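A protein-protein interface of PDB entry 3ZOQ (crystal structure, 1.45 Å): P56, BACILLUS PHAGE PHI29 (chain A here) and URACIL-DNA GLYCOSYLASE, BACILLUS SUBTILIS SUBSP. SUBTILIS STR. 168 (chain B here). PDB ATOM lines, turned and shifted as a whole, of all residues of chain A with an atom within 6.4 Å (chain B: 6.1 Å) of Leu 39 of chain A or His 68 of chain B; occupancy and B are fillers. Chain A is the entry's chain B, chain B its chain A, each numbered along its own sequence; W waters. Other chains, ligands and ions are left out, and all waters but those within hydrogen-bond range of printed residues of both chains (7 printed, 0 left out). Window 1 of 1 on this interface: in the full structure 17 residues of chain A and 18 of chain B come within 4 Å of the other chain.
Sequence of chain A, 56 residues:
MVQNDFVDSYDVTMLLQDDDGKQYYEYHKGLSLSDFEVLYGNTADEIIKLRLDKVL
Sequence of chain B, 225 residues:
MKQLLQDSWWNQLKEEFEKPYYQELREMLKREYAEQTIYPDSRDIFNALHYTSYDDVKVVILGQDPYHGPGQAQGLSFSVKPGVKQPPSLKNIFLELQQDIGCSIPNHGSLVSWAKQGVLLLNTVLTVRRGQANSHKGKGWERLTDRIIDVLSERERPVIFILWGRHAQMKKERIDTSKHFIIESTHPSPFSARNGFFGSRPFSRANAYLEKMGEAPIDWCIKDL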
ATOM      1  N   VAL A  12      -5.452 -35.376 -25.657  1.00  0.00           N
ATOM      2  CA  VAL A  12      -5.655 -34.036 -26.220  1.00  0.00           C
ATOM      3  C   VAL A  12      -4.326 -33.473 -26.659  1.00  0.00           C
ATOM      4  O   VAL A  12      -3.406 -33.348 -25.844  1.00  0.00           O
ATOM      5  CB  VAL A  12      -6.257 -33.063 -25.175  1.00  0.00           C
ATOM      6  CG1 VAL A  12      -6.562 -31.706 -25.801  1.00  0.00           C
ATOM      7  CG2 VAL A  12      -7.502 -33.657 -24.535  1.00  0.00           C
ATOM      8  N   MET A  14      -2.560 -30.138 -28.604  1.00  0.00           N
ATOM      9  CA  MET A  14      -2.754 -28.780 -29.099  1.00  0.00           C
ATOM     10  C   MET A  14      -1.476 -28.195 -29.670  1.00  0.00           C
ATOM     11  O   MET A  14      -0.400 -28.383 -29.097  1.00  0.00           O
ATOM     12  CB  MET A  14      -3.271 -27.878 -27.984  1.00  0.00           C
ATOM     13  CG  MET A  14      -4.698 -28.199 -27.592  1.00  0.00           C
ATOM     14  SD  MET A  14      -5.365 -27.100 -26.339  1.00  0.00           S
ATOM     15  CE  MET A  14      -4.490 -27.706 -24.907  1.00  0.00           C
ATOM     16  N   GLU A  26       1.503 -29.173 -27.190  1.00  0.00           N
ATOM     17  CA  GLU A  26       1.286 -29.730 -25.835  1.00  0.00           C
ATOM     18  C   GLU A  26       0.548 -31.059 -25.985  1.00  0.00           C
ATOM     19  O   GLU A  26      -0.338 -31.193 -26.839  1.00  0.00           O
ATOM     20  CB  GLU A  26       0.377 -28.836 -24.987  1.00  0.00           C
ATOM     21  CG  GLU A  26       0.993 -27.590 -24.383  1.00  0.00           C
ATOM     22  CD  GLU A  26       0.041 -26.876 -23.431  1.00  0.00           C
ATOM     23  OE1 GLU A  26      -1.162 -27.255 -23.335  1.00  0.00           O
ATOM     24  OE2 GLU A  26       0.498 -25.916 -22.775  1.00  0.00           O
ATOM     25  N   HIS A  28      -1.623 -33.843 -23.770  1.00  0.00           N
ATOM     26  CA  HIS A  28      -2.283 -34.253 -22.529  1.00  0.00           C
ATOM     27  C   HIS A  28      -2.878 -35.612 -22.730  1.00  0.00           C
ATOM     28  O   HIS A  28      -3.380 -35.915 -23.808  1.00  0.00           O
ATOM     29  CB  HIS A  28      -3.351 -33.235 -22.143  1.00  0.00           C
ATOM     30  CG  HIS A  28      -2.831 -31.824 -22.060  1.00  0.00           C
ATOM     31  ND1 HIS A  28      -2.388 -31.282 -20.914  1.00  0.00           N
ATOM     32  CD2 HIS A  28      -2.676 -30.846 -23.043  1.00  0.00           C
ATOM     33  CE1 HIS A  28      -1.976 -30.022 -21.142  1.00  0.00           C
ATOM     34  NE2 HIS A  28      -2.153 -29.757 -22.447  1.00  0.00           N
ATOM     35  N   LEU A  31      -7.626 -37.897 -20.368  1.00  0.00           N
ATOM     36  CA  LEU A  31      -8.607 -36.949 -19.859  1.00  0.00           C
ATOM     37  C   LEU A  31     -10.031 -37.397 -20.164  1.00  0.00           C
ATOM     38  O   LEU A  31     -10.318 -37.937 -21.240  1.00  0.00           O
ATOM     39  CB  LEU A  31      -8.370 -35.573 -20.488  1.00  0.00           C
ATOM     40  CG  LEU A  31      -7.355 -34.677 -19.769  1.00  0.00           C
ATOM     41  CD1 LEU A  31      -5.930 -35.212 -19.791  1.00  0.00           C
ATOM     42  CD2 LEU A  31      -7.376 -33.270 -20.347  1.00  0.00           C
ATOM     43  N   SER A  34     -15.042 -33.954 -19.584  1.00  0.00           N
ATOM     44  CA  SER A  34     -15.127 -32.865 -18.620  1.00  0.00           C
ATOM     45  C   SER A  34     -13.753 -32.244 -18.367  1.00  0.00           C
ATOM     46  O   SER A  34     -13.617 -31.014 -18.384  1.00  0.00           O
ATOM     47  CB  SER A  34     -15.776 -33.342 -17.319  1.00  0.00           C
ATOM     48  OG  SER A  34     -17.124 -33.716 -17.546  1.00  0.00           O
ATOM     49  N   ASP A  35     -12.734 -33.087 -18.178  1.00  0.00           N
ATOM     50  CA  ASP A  35     -11.353 -32.596 -17.988  1.00  0.00           C
ATOM     51  C   ASP A  35     -10.903 -31.805 -19.214  1.00  0.00           C
ATOM     52  O   ASP A  35     -10.223 -30.791 -19.075  1.00  0.00           O
ATOM     53  CB  ASP A  35     -10.349 -33.743 -17.808  1.00  0.00           C
ATOM     54  CG  ASP A  35     -10.583 -34.575 -16.567  1.00  0.00           C
ATOM     55  OD1 ASP A  35     -11.181 -34.093 -15.581  1.00  0.00           O
ATOM     56  OD2 ASP A  35     -10.120 -35.740 -16.594  1.00  0.00           O
ATOM     57  N   PHE A  36     -11.260 -32.289 -20.405  1.00  0.00           N
ATOM     58  CA  PHE A  36     -10.910 -31.591 -21.641  1.00  0.00           C
ATOM     59  C   PHE A  36     -11.540 -30.185 -21.681  1.00  0.00           C
ATOM     60  O   PHE A  36     -10.878 -29.214 -22.051  1.00  0.00           O
ATOM     61  CB  PHE A  36     -11.319 -32.406 -22.880  1.00  0.00           C
ATOM     62  CG  PHE A  36     -11.411 -31.574 -24.132  1.00  0.00           C
ATOM     63  CD1 PHE A  36     -10.258 -30.989 -24.670  1.00  0.00           C
ATOM     64  CD2 PHE A  36     -12.647 -31.320 -24.733  1.00  0.00           C
ATOM     65  CE1 PHE A  36     -10.332 -30.190 -25.804  1.00  0.00           C
ATOM     66  CE2 PHE A  36     -12.724 -30.528 -25.873  1.00  0.00           C
ATOM     67  CZ  PHE A  36     -11.566 -29.966 -26.405  1.00  0.00           C
ATOM     68  N   GLU A  37     -12.815 -30.084 -21.307  1.00  0.00           N
ATOM     69  CA  GLU A  37     -13.520 -28.805 -21.334  1.00  0.00           C
ATOM     70  C   GLU A  37     -12.859 -27.809 -20.372  1.00  0.00           C
ATOM     71  O   GLU A  37     -12.692 -26.621 -20.685  1.00  0.00           O
ATOM     72  CB  GLU A  37     -15.014 -29.007 -21.029  1.00  0.00           C
ATOM     73  CG  GLU A  37     -15.715 -29.816 -22.109  1.00  0.00           C
ATOM     74  CD  GLU A  37     -16.936 -30.584 -21.627  1.00  0.00           C
ATOM     75  OE1 GLU A  37     -17.394 -30.379 -20.484  1.00  0.00           O
ATOM     76  OE2 GLU A  37     -17.443 -31.406 -22.405  1.00  0.00           O
ATOM     77  N   VAL A  38     -12.446 -28.302 -19.213  1.00  0.00           N
ATOM     78  CA  VAL A  38     -11.713 -27.465 -18.261  1.00  0.00           C
ATOM     79  C   VAL A  38     -10.333 -27.068 -18.822  1.00  0.00           C
ATOM     80  O   VAL A  38      -9.927 -25.906 -18.736  1.00  0.00           O
ATOM     81  CB  VAL A  38     -11.603 -28.181 -16.895  1.00  0.00           C
ATOM     82  CG1 VAL A  38     -10.733 -27.393 -15.931  1.00  0.00           C
ATOM     83  CG2 VAL A  38     -12.985 -28.343 -16.288  1.00  0.00           C
ATOM     84  N   LEU A  39      -9.622 -28.033 -19.408  1.00  0.00           N
ATOM     85  CA  LEU A  39      -8.303 -27.781 -20.009  1.00  0.00           C
ATOM     86  C   LEU A  39      -8.376 -26.676 -21.068  1.00  0.00           C
ATOM     87  O   LEU A  39      -7.534 -25.770 -21.092  1.00  0.00           O
ATOM     88  CB  LEU A  39      -7.725 -29.072 -20.606  1.00  0.00           C
ATOM     89  CG  LEU A  39      -6.528 -28.917 -21.564  1.00  0.00           C
ATOM     90  CD1 LEU A  39      -5.300 -28.319 -20.881  1.00  0.00           C
ATOM     91  CD2 LEU A  39      -6.195 -30.270 -22.188  1.00  0.00           C
ATOM     92  N   TYR A  40      -9.401 -26.740 -21.916  1.00  0.00           N
ATOM     93  CA  TYR A  40      -9.593 -25.736 -22.965  1.00  0.00           C
ATOM     94  C   TYR A  40      -9.703 -24.331 -22.347  1.00  0.00           C
ATOM     95  O   TYR A  40      -9.040 -23.369 -22.795  1.00  0.00           O
ATOM     96  CB  TYR A  40     -10.840 -26.094 -23.756  1.00  0.00           C
ATOM     97  CG  TYR A  40     -11.177 -25.176 -24.908  1.00  0.00           C
ATOM     98  CD1 TYR A  40     -10.547 -25.315 -26.148  1.00  0.00           C
ATOM     99  CD2 TYR A  40     -12.185 -24.219 -24.789  1.00  0.00           C
ATOM    100  CE1 TYR A  40     -10.888 -24.497 -27.226  1.00  0.00           C
ATOM    101  CE2 TYR A  40     -12.532 -23.403 -25.859  1.00  0.00           C
ATOM    102  CZ  TYR A  40     -11.882 -23.552 -27.073  1.00  0.00           C
ATOM    103  OH  TYR A  40     -12.220 -22.762 -28.145  1.00  0.00           O
ATOM    104  N   GLY A  41     -10.487 -24.223 -21.272  1.00  0.00           N
ATOM    105  CA  GLY A  41     -10.604 -22.948 -20.529  1.00  0.00           C
ATOM    106  C   GLY A  41      -9.355 -22.526 -19.759  1.00  0.00           C
ATOM    107  O   GLY A  41      -9.251 -21.382 -19.312  1.00  0.00           O
ATOM    108  N   ASN A  42      -8.401 -23.454 -19.607  1.00  0.00           N
ATOM    109  CA  ASN A  42      -7.126 -23.175 -18.921  1.00  0.00           C
ATOM    110  C   ASN A  42      -5.964 -22.995 -19.882  1.00  0.00           C
ATOM    111  O   ASN A  42      -4.812 -23.000 -19.455  1.00  0.00           O
ATOM    112  CB  ASN A  42      -6.769 -24.302 -17.949  1.00  0.00           C
ATOM    113  CG  ASN A  42      -7.655 -24.335 -16.736  1.00  0.00           C
ATOM    114  OD1 ASN A  42      -8.358 -23.370 -16.435  1.00  0.00           O
ATOM    115  ND2 ASN A  42      -7.632 -25.468 -16.031  1.00  0.00           N
ATOM    116  N   THR A  43      -6.269 -22.865 -21.171  1.00  0.00           N
ATOM    117  CA  THR A  43      -5.247 -22.715 -22.216  1.00  0.00           C
ATOM    118  C   THR A  43      -5.127 -21.241 -22.601  1.00  0.00           C
ATOM    119  O   THR A  43      -6.025 -20.700 -23.258  1.00  0.00           O
ATOM    120  CB  THR A  43      -5.603 -23.599 -23.427  1.00  0.00           C
ATOM    121  OG1 THR A  43      -5.630 -24.970 -23.003  1.00  0.00           O
ATOM    122  CG2 THR A  43      -4.585 -23.434 -24.550  1.00  0.00           C
ATOM    123  N   ALA A  44      -4.040 -20.590 -22.173  1.00  0.00           N
ATOM    124  CA  ALA A  44      -3.928 -19.134 -22.323  1.00  0.00           C
ATOM    125  C   ALA A  44      -3.424 -18.639 -23.673  1.00  0.00           C
ATOM    126  O   ALA A  44      -3.809 -17.558 -24.107  1.00  0.00           O
ATOM    127  CB  ALA A  44      -3.087 -18.540 -21.210  1.00  0.00           C
ATOM    128  N   TYR B  39       3.938 -27.816 -10.685  1.00  0.00           N
ATOM    129  CA  TYR B  39       3.279 -26.577 -10.292  1.00  0.00           C
ATOM    130  C   TYR B  39       2.184 -26.837  -9.248  1.00  0.00           C
ATOM    131  O   TYR B  39       1.593 -27.912  -9.232  1.00  0.00           O
ATOM    132  CB  TYR B  39       2.681 -25.871 -11.514  1.00  0.00           C
ATOM    133  CG  TYR B  39       3.697 -25.475 -12.563  1.00  0.00           C
ATOM    134  CD1 TYR B  39       4.816 -24.719 -12.231  1.00  0.00           C
ATOM    135  CD2 TYR B  39       3.517 -25.845 -13.885  1.00  0.00           C
ATOM    136  CE1 TYR B  39       5.744 -24.351 -13.196  1.00  0.00           C
ATOM    137  CE2 TYR B  39       4.434 -25.479 -14.853  1.00  0.00           C
ATOM    138  CZ  TYR B  39       5.548 -24.733 -14.507  1.00  0.00           C
ATOM    139  OH  TYR B  39       6.470 -24.376 -15.477  1.00  0.00           O
ATOM    140  N   PRO B  66      -4.254 -27.509 -10.482  1.00  0.00           N
ATOM    141  CA  PRO B  66      -3.578 -26.238 -10.761  1.00  0.00           C
ATOM    142  C   PRO B  66      -3.317 -26.011 -12.245  1.00  0.00           C
ATOM    143  O   PRO B  66      -3.177 -26.962 -13.016  1.00  0.00           O
ATOM    144  CB  PRO B  66      -2.235 -26.381 -10.031  1.00  0.00           C
ATOM    145  CG  PRO B  66      -2.452 -27.458  -9.021  1.00  0.00           C
ATOM    146  CD  PRO B  66      -3.392 -28.413  -9.691  1.00  0.00           C
ATOM    147  N   TYR B  67      -3.197 -24.747 -12.639  1.00  0.00           N
ATOM    148  CA  TYR B  67      -2.699 -24.443 -13.978  1.00  0.00           C
ATOM    149  C   TYR B  67      -1.347 -25.121 -14.205  1.00  0.00           C
ATOM    150  O   TYR B  67      -0.519 -25.201 -13.291  1.00  0.00           O
ATOM    151  CB  TYR B  67      -2.540 -22.933 -14.136  1.00  0.00           C
ATOM    152  CG  TYR B  67      -3.839 -22.160 -14.124  1.00  0.00           C
ATOM    153  CD1 TYR B  67      -4.764 -22.294 -15.164  1.00  0.00           C
ATOM    154  CD2 TYR B  67      -4.141 -21.291 -13.084  1.00  0.00           C
ATOM    155  CE1 TYR B  67      -5.954 -21.578 -15.167  1.00  0.00           C
ATOM    156  CE2 TYR B  67      -5.335 -20.570 -13.079  1.00  0.00           C
ATOM    157  CZ  TYR B  67      -6.233 -20.720 -14.126  1.00  0.00           C
ATOM    158  OH  TYR B  67      -7.417 -20.015 -14.164  1.00  0.00           O
ATOM    159  N   HIS B  68      -1.132 -25.594 -15.432  1.00  0.00           N
ATOM    160  CA  HIS B  68       0.019 -26.455 -15.739  1.00  0.00           C
ATOM    161  C   HIS B  68       1.111 -25.754 -16.531  1.00  0.00           C
ATOM    162  O   HIS B  68       2.064 -26.397 -16.979  1.00  0.00           O
ATOM    163  CB  HIS B  68      -0.459 -27.697 -16.484  1.00  0.00           C
ATOM    164  CG  HIS B  68      -1.107 -27.364 -17.793  1.00  0.00           C
ATOM    165  ND1 HIS B  68      -2.442 -27.371 -17.972  1.00  0.00           N
ATOM    166  CD2 HIS B  68      -0.549 -26.909 -18.990  1.00  0.00           C
ATOM    167  CE1 HIS B  68      -2.718 -26.971 -19.230  1.00  0.00           C
ATOM    168  NE2 HIS B  68      -1.562 -26.697 -19.848  1.00  0.00           N
ATOM    169  N   GLY B  69       1.003 -24.436 -16.706  1.00  0.00           N
ATOM    170  CA  GLY B  69       2.012 -23.680 -17.457  1.00  0.00           C
ATOM    171  C   GLY B  69       2.903 -22.795 -16.599  1.00  0.00           C
ATOM    172  O   GLY B  69       2.536 -22.438 -15.478  1.00  0.00           O
ATOM    173  N   PRO B  70       4.072 -22.401 -17.127  1.00  0.00           N
ATOM    174  CA  PRO B  70       4.983 -21.597 -16.309  1.00  0.00           C
ATOM    175  C   PRO B  70       4.363 -20.279 -15.874  1.00  0.00           C
ATOM    176  O   PRO B  70       3.649 -19.633 -16.657  1.00  0.00           O
ATOM    177  CB  PRO B  70       6.189 -21.349 -17.235  1.00  0.00           C
ATOM    178  CG  PRO B  70       5.766 -21.796 -18.584  1.00  0.00           C
ATOM    179  CD  PRO B  70       4.693 -22.815 -18.399  1.00  0.00           C
ATOM    180  N   GLN B  72       1.955 -19.538 -13.848  1.00  0.00           N
ATOM    181  CA  GLN B  72       0.503 -19.418 -13.672  1.00  0.00           C
ATOM    182  C   GLN B  72       0.025 -19.698 -12.237  1.00  0.00           C
ATOM    183  O   GLN B  72      -0.452 -18.789 -11.557  1.00  0.00           O
ATOM    184  CB  GLN B  72      -0.237 -20.305 -14.672  1.00  0.00           C
ATOM    185  CG  GLN B  72      -0.025 -19.911 -16.140  1.00  0.00           C
ATOM    186  CD  GLN B  72      -0.750 -20.847 -17.091  1.00  0.00           C
ATOM    187  OE1 GLN B  72      -0.762 -22.069 -16.894  1.00  0.00           O
ATOM    188  NE2 GLN B  72      -1.370 -20.283 -18.122  1.00  0.00           N
ATOM    189  N   ALA B  73       0.147 -20.948 -11.793  1.00  0.00           N
ATOM    190  CA  ALA B  73      -0.476 -21.388 -10.534  1.00  0.00           C
ATOM    191  C   ALA B  73       0.162 -20.789  -9.288  1.00  0.00           C
ATOM    192  O   ALA B  73       1.394 -20.705  -9.178  1.00  0.00           O
ATOM    193  CB  ALA B  73      -0.440 -22.898 -10.430  1.00  0.00           C
ATOM    194  N   VAL B 128       0.478 -30.450 -10.140  1.00  0.00           N
ATOM    195  CA  VAL B 128       0.376 -30.942 -11.519  1.00  0.00           C
ATOM    196  C   VAL B 128       1.768 -30.911 -12.160  1.00  0.00           C
ATOM    197  O   VAL B 128       2.583 -30.062 -11.818  1.00  0.00           O
ATOM    198  CB  VAL B 128      -0.620 -30.078 -12.344  1.00  0.00           C
ATOM    199  CG1 VAL B 128      -0.093 -28.650 -12.557  1.00  0.00           C
ATOM    200  CG2 VAL B 128      -0.974 -30.757 -13.664  1.00  0.00           C
ATOM    201  N   ARG B 129       2.036 -31.854 -13.065  1.00  0.00           N
ATOM    202  CA  ARG B 129       3.253 -31.811 -13.877  1.00  0.00           C
ATOM    203  C   ARG B 129       3.082 -30.775 -14.991  1.00  0.00           C
ATOM    204  O   ARG B 129       2.027 -30.707 -15.622  1.00  0.00           O
ATOM    205  CB  ARG B 129       3.562 -33.190 -14.486  1.00  0.00           C
ATOM    206  CG  ARG B 129       3.700 -34.323 -13.475  1.00  0.00           C
ATOM    207  CD  ARG B 129       3.818 -35.704 -14.132  1.00  0.00           C
ATOM    208  NE  ARG B 129       3.959 -36.734 -13.098  1.00  0.00           N
ATOM    209  CZ  ARG B 129       3.390 -37.935 -13.132  1.00  0.00           C
ATOM    210  NH1 ARG B 129       2.647 -38.294 -14.168  1.00  0.00           N
ATOM    211  NH2 ARG B 129       3.574 -38.778 -12.121  1.00  0.00           N
ATOM    212  N   ARG B 130       4.124 -29.977 -15.230  1.00  0.00           N
ATOM    213  CA  ARG B 130       4.099 -29.003 -16.322  1.00  0.00           C
ATOM    214  C   ARG B 130       3.598 -29.604 -17.637  1.00  0.00           C
ATOM    215  O   ARG B 130       4.066 -30.672 -18.066  1.00  0.00           O
ATOM    216  CB  ARG B 130       5.490 -28.403 -16.545  1.00  0.00           C
ATOM    217  CG  ARG B 130       5.546 -27.514 -17.773  1.00  0.00           C
ATOM    218  CD  ARG B 130       6.872 -26.798 -17.930  1.00  0.00           C
ATOM    219  NE  ARG B 130       6.864 -26.061 -19.195  1.00  0.00           N
ATOM    220  CZ  ARG B 130       7.672 -25.052 -19.500  1.00  0.00           C
ATOM    221  NH1 ARG B 130       8.602 -24.647 -18.642  1.00  0.00           N
ATOM    222  NH2 ARG B 130       7.536 -24.433 -20.669  1.00  0.00           N
ATOM    223  N   GLY B 131       2.643 -28.902 -18.263  1.00  0.00           N
ATOM    224  CA  GLY B 131       2.130 -29.262 -19.594  1.00  0.00           C
ATOM    225  C   GLY B 131       1.317 -30.541 -19.674  1.00  0.00           C
ATOM    226  O   GLY B 131       1.040 -31.028 -20.774  1.00  0.00           O
ATOM    227  N   GLN B 132       0.922 -31.087 -18.516  1.00  0.00           N
ATOM    228  CA  GLN B 132       0.235 -32.379 -18.480  1.00  0.00           C
ATOM    229  C   GLN B 132      -0.971 -32.334 -17.549  1.00  0.00           C
ATOM    230  O   GLN B 132      -0.887 -32.696 -16.372  1.00  0.00           O
ATOM    231  CB  GLN B 132       1.207 -33.498 -18.081  1.00  0.00           C
ATOM    232  CG  GLN B 132       2.444 -33.579 -18.965  1.00  0.00           C
ATOM    233  CD  GLN B 132       3.484 -34.524 -18.423  1.00  0.00           C
ATOM    234  OE1 GLN B 132       3.373 -35.740 -18.569  1.00  0.00           O
ATOM    235  NE2 GLN B 132       4.512 -33.969 -17.799  1.00  0.00           N
ATOM    236  N   ALA B 133      -2.099 -31.885 -18.080  1.00  0.00           N
ATOM    237  CA  ALA B 133      -3.270 -31.687 -17.251  1.00  0.00           C
ATOM    238  C   ALA B 133      -3.682 -32.981 -16.575  1.00  0.00           C
ATOM    239  O   ALA B 133      -3.609 -34.037 -17.178  1.00  0.00           O
ATOM    240  CB  ALA B 133      -4.414 -31.134 -18.087  1.00  0.00           C
ATOM    241  N   ASN B 134      -4.113 -32.865 -15.316  1.00  0.00           N
ATOM    242  CA  ASN B 134      -4.669 -33.982 -14.537  1.00  0.00           C
ATOM    243  C   ASN B 134      -3.647 -35.101 -14.262  1.00  0.00           C
ATOM    244  O   ASN B 134      -4.012 -36.213 -13.872  1.00  0.00           O
ATOM    245  CB  ASN B 134      -6.014 -34.454 -15.141  1.00  0.00           C
ATOM    246  CG  ASN B 134      -6.977 -33.292 -15.379  1.00  0.00           C
ATOM    247  OD1 ASN B 134      -7.605 -32.785 -14.446  1.00  0.00           O
ATOM    248  ND2 ASN B 134      -7.069 -32.840 -16.626  1.00  0.00           N
HETATM  249  O   HOH W   1      -9.275 -22.229 -14.043  1.00  0.00           O
HETATM  250  O   HOH W   2      -8.831 -20.008 -16.641  1.00  0.00           O
HETATM  251  O   HOH W   3       2.222 -25.840 -20.184  1.00  0.00           O
HETATM  252  O   HOH W   4      -3.115 -25.728 -22.049  1.00  0.00           O
HETATM  253  O   HOH W   5      -8.119 -30.322 -17.176  1.00  0.00           O
HETATM  254  O   HOH W   6      -2.703 -23.995 -17.456  1.00  0.00           O
HETATM  255  O   HOH W   7      -2.340 -22.022 -20.282  1.00  0.00           O
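The backbone carbonyl oxygen (O) of Gly 131 of chain B lies close to a ring nitrogen (ND1) of His 28 of chain A (3.4 Å).
The backbone NH (N) of Ala 133 of chain B sits at hydrogen-bond distance from a ring nitrogen (ND1) of His 28 of chain A (2.9 Å).
The backbone carbonyl oxygen (O) of His 68 of chain B lies within hydrogen-bond range of the backbone NH (N) of Gly 131 of chain B (2.9 Å).
The backbone NH (N) of Gly 69 of chain B sits at hydrogen-bond distance from the side-chain amide oxygen (OE1) of Gln 72 of chain B (3.0 Å).
The backbone carbonyl oxygen of Arg 130 of chain B is in hydrogen-bond range of the side-chain amide nitrogen of Gln 132 of chain B, 3.3 Å away.
The backbone NH (N) of His 28 of chain A lies within hydrogen-bond range of the backbone carbonyl oxygen (O) of Val 12 of chain A, at 2.8 Å.
The backbone carbonyl oxygen (O) of Met 14 of chain A lies within hydrogen-bond range of the backbone NH (N) of Glu 26 of chain A (2.8 Å).
NE2 of His 28 of chain A lies within hydrogen-bond range of OE1 of Glu 26 of chain A, at 2.8 Å.
Glu 26 of chain A touches His 68 of chain B (OE1 to NE2, 3.6 Å).
His 28 of chain A touches His 68 of chain B.
His 28 of chain A touches Gln 132 of chain B.
O of Ala 133 of chain B touches CD1 of Leu 31 of chain A (3.7 Å).
CG of Leu 31 of chain A touches ND2 of Asn 134 of chain B (3.7 Å).
Asn 134 of chain B touches Asp 35 of chain A (ND2 to CB, 3.6 Å).
Leu 39 of chain A touches His 68 of chain B (CD1 to CE1, 3.3 Å).
OD1 of Asn 42 of chain A touches CE1 of Tyr 67 of chain B, 3.3 Å away.
Gln 72 of chain B touches Ala 44 of chain A (NE2 to CB, 3.9 Å).
Of chain B, only His 68 comes within 4 Å of Leu 39 of chain A.
Of chain A, only Glu 26 (3.6 Å), His 28 (3.6 Å) and Leu 39 (3.3 Å) come within 4 Å of His 68 of chain B.
Of the printed residues of chain A, Gln 132 of chain B touches His 28.
Of the printed residues of chain A, Tyr 67 of chain B touches Asn 42.
Val 12 of chain A touches none of the printed residues of chain B.
The nearest residue of chain A that does not touch His 68 of chain B is Asn 42 of chain A (4.5 Å).
Hydrophobic or aromatic side chains of chain A that line the printed part of chain B: His 28, Leu 31, Leu 39 and Ala 44.
Hydrophobic or aromatic side chains of chain B within 4 Å of the printed part of chain A: Tyr 67, His 68 and Ala 133.
Among the printed residues, no Asp or Glu carboxylate lies within 4 Å of a Lys or Arg side-chain nitrogen of the other chain.
Water W5 bridges ND2 of Asn 134 of chain B (2.8 Å) and O of Asp 35 of chain A (2.9 Å).
Water W7 lies within hydrogen-bond range of O of Asn 42 of chain A (2.8 Å), N of Ala 44 of chain A (2.9 Å) and NE2 of Gln 72 of chain B (2.9 Å).
Water W6 lies within hydrogen-bond range of the side-chain amide oxygen of Gln 72 of chain B (2.8 Å), the backbone NH of His 68 of chain B (3.0 Å) and the backbone carbonyl oxygen of Asn 42 of chain A (3.1 Å).
Water W4 lies within hydrogen-bond range of OE1 of Glu 26 of chain A (2.8 Å), OG1 of Thr 43 of chain A (2.8 Å) and NE2 of His 68 of chain B (2.9 Å).
Water W1 lies within hydrogen-bond range of the side-chain amide oxygen (OD1) of Asn 42 of chain A (2.8 Å) and the side-chain hydroxyl (OH) of Tyr 67 of chain B (2.9 Å).
Water W2 lies within hydrogen-bond range of the side-chain hydroxyl of Tyr 67 of chain B (2.9 Å), the backbone carbonyl oxygen of Gly 41 of chain A (3.0 Å) and the side-chain amide oxygen of Asn 42 of chain A (3.4 Å).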
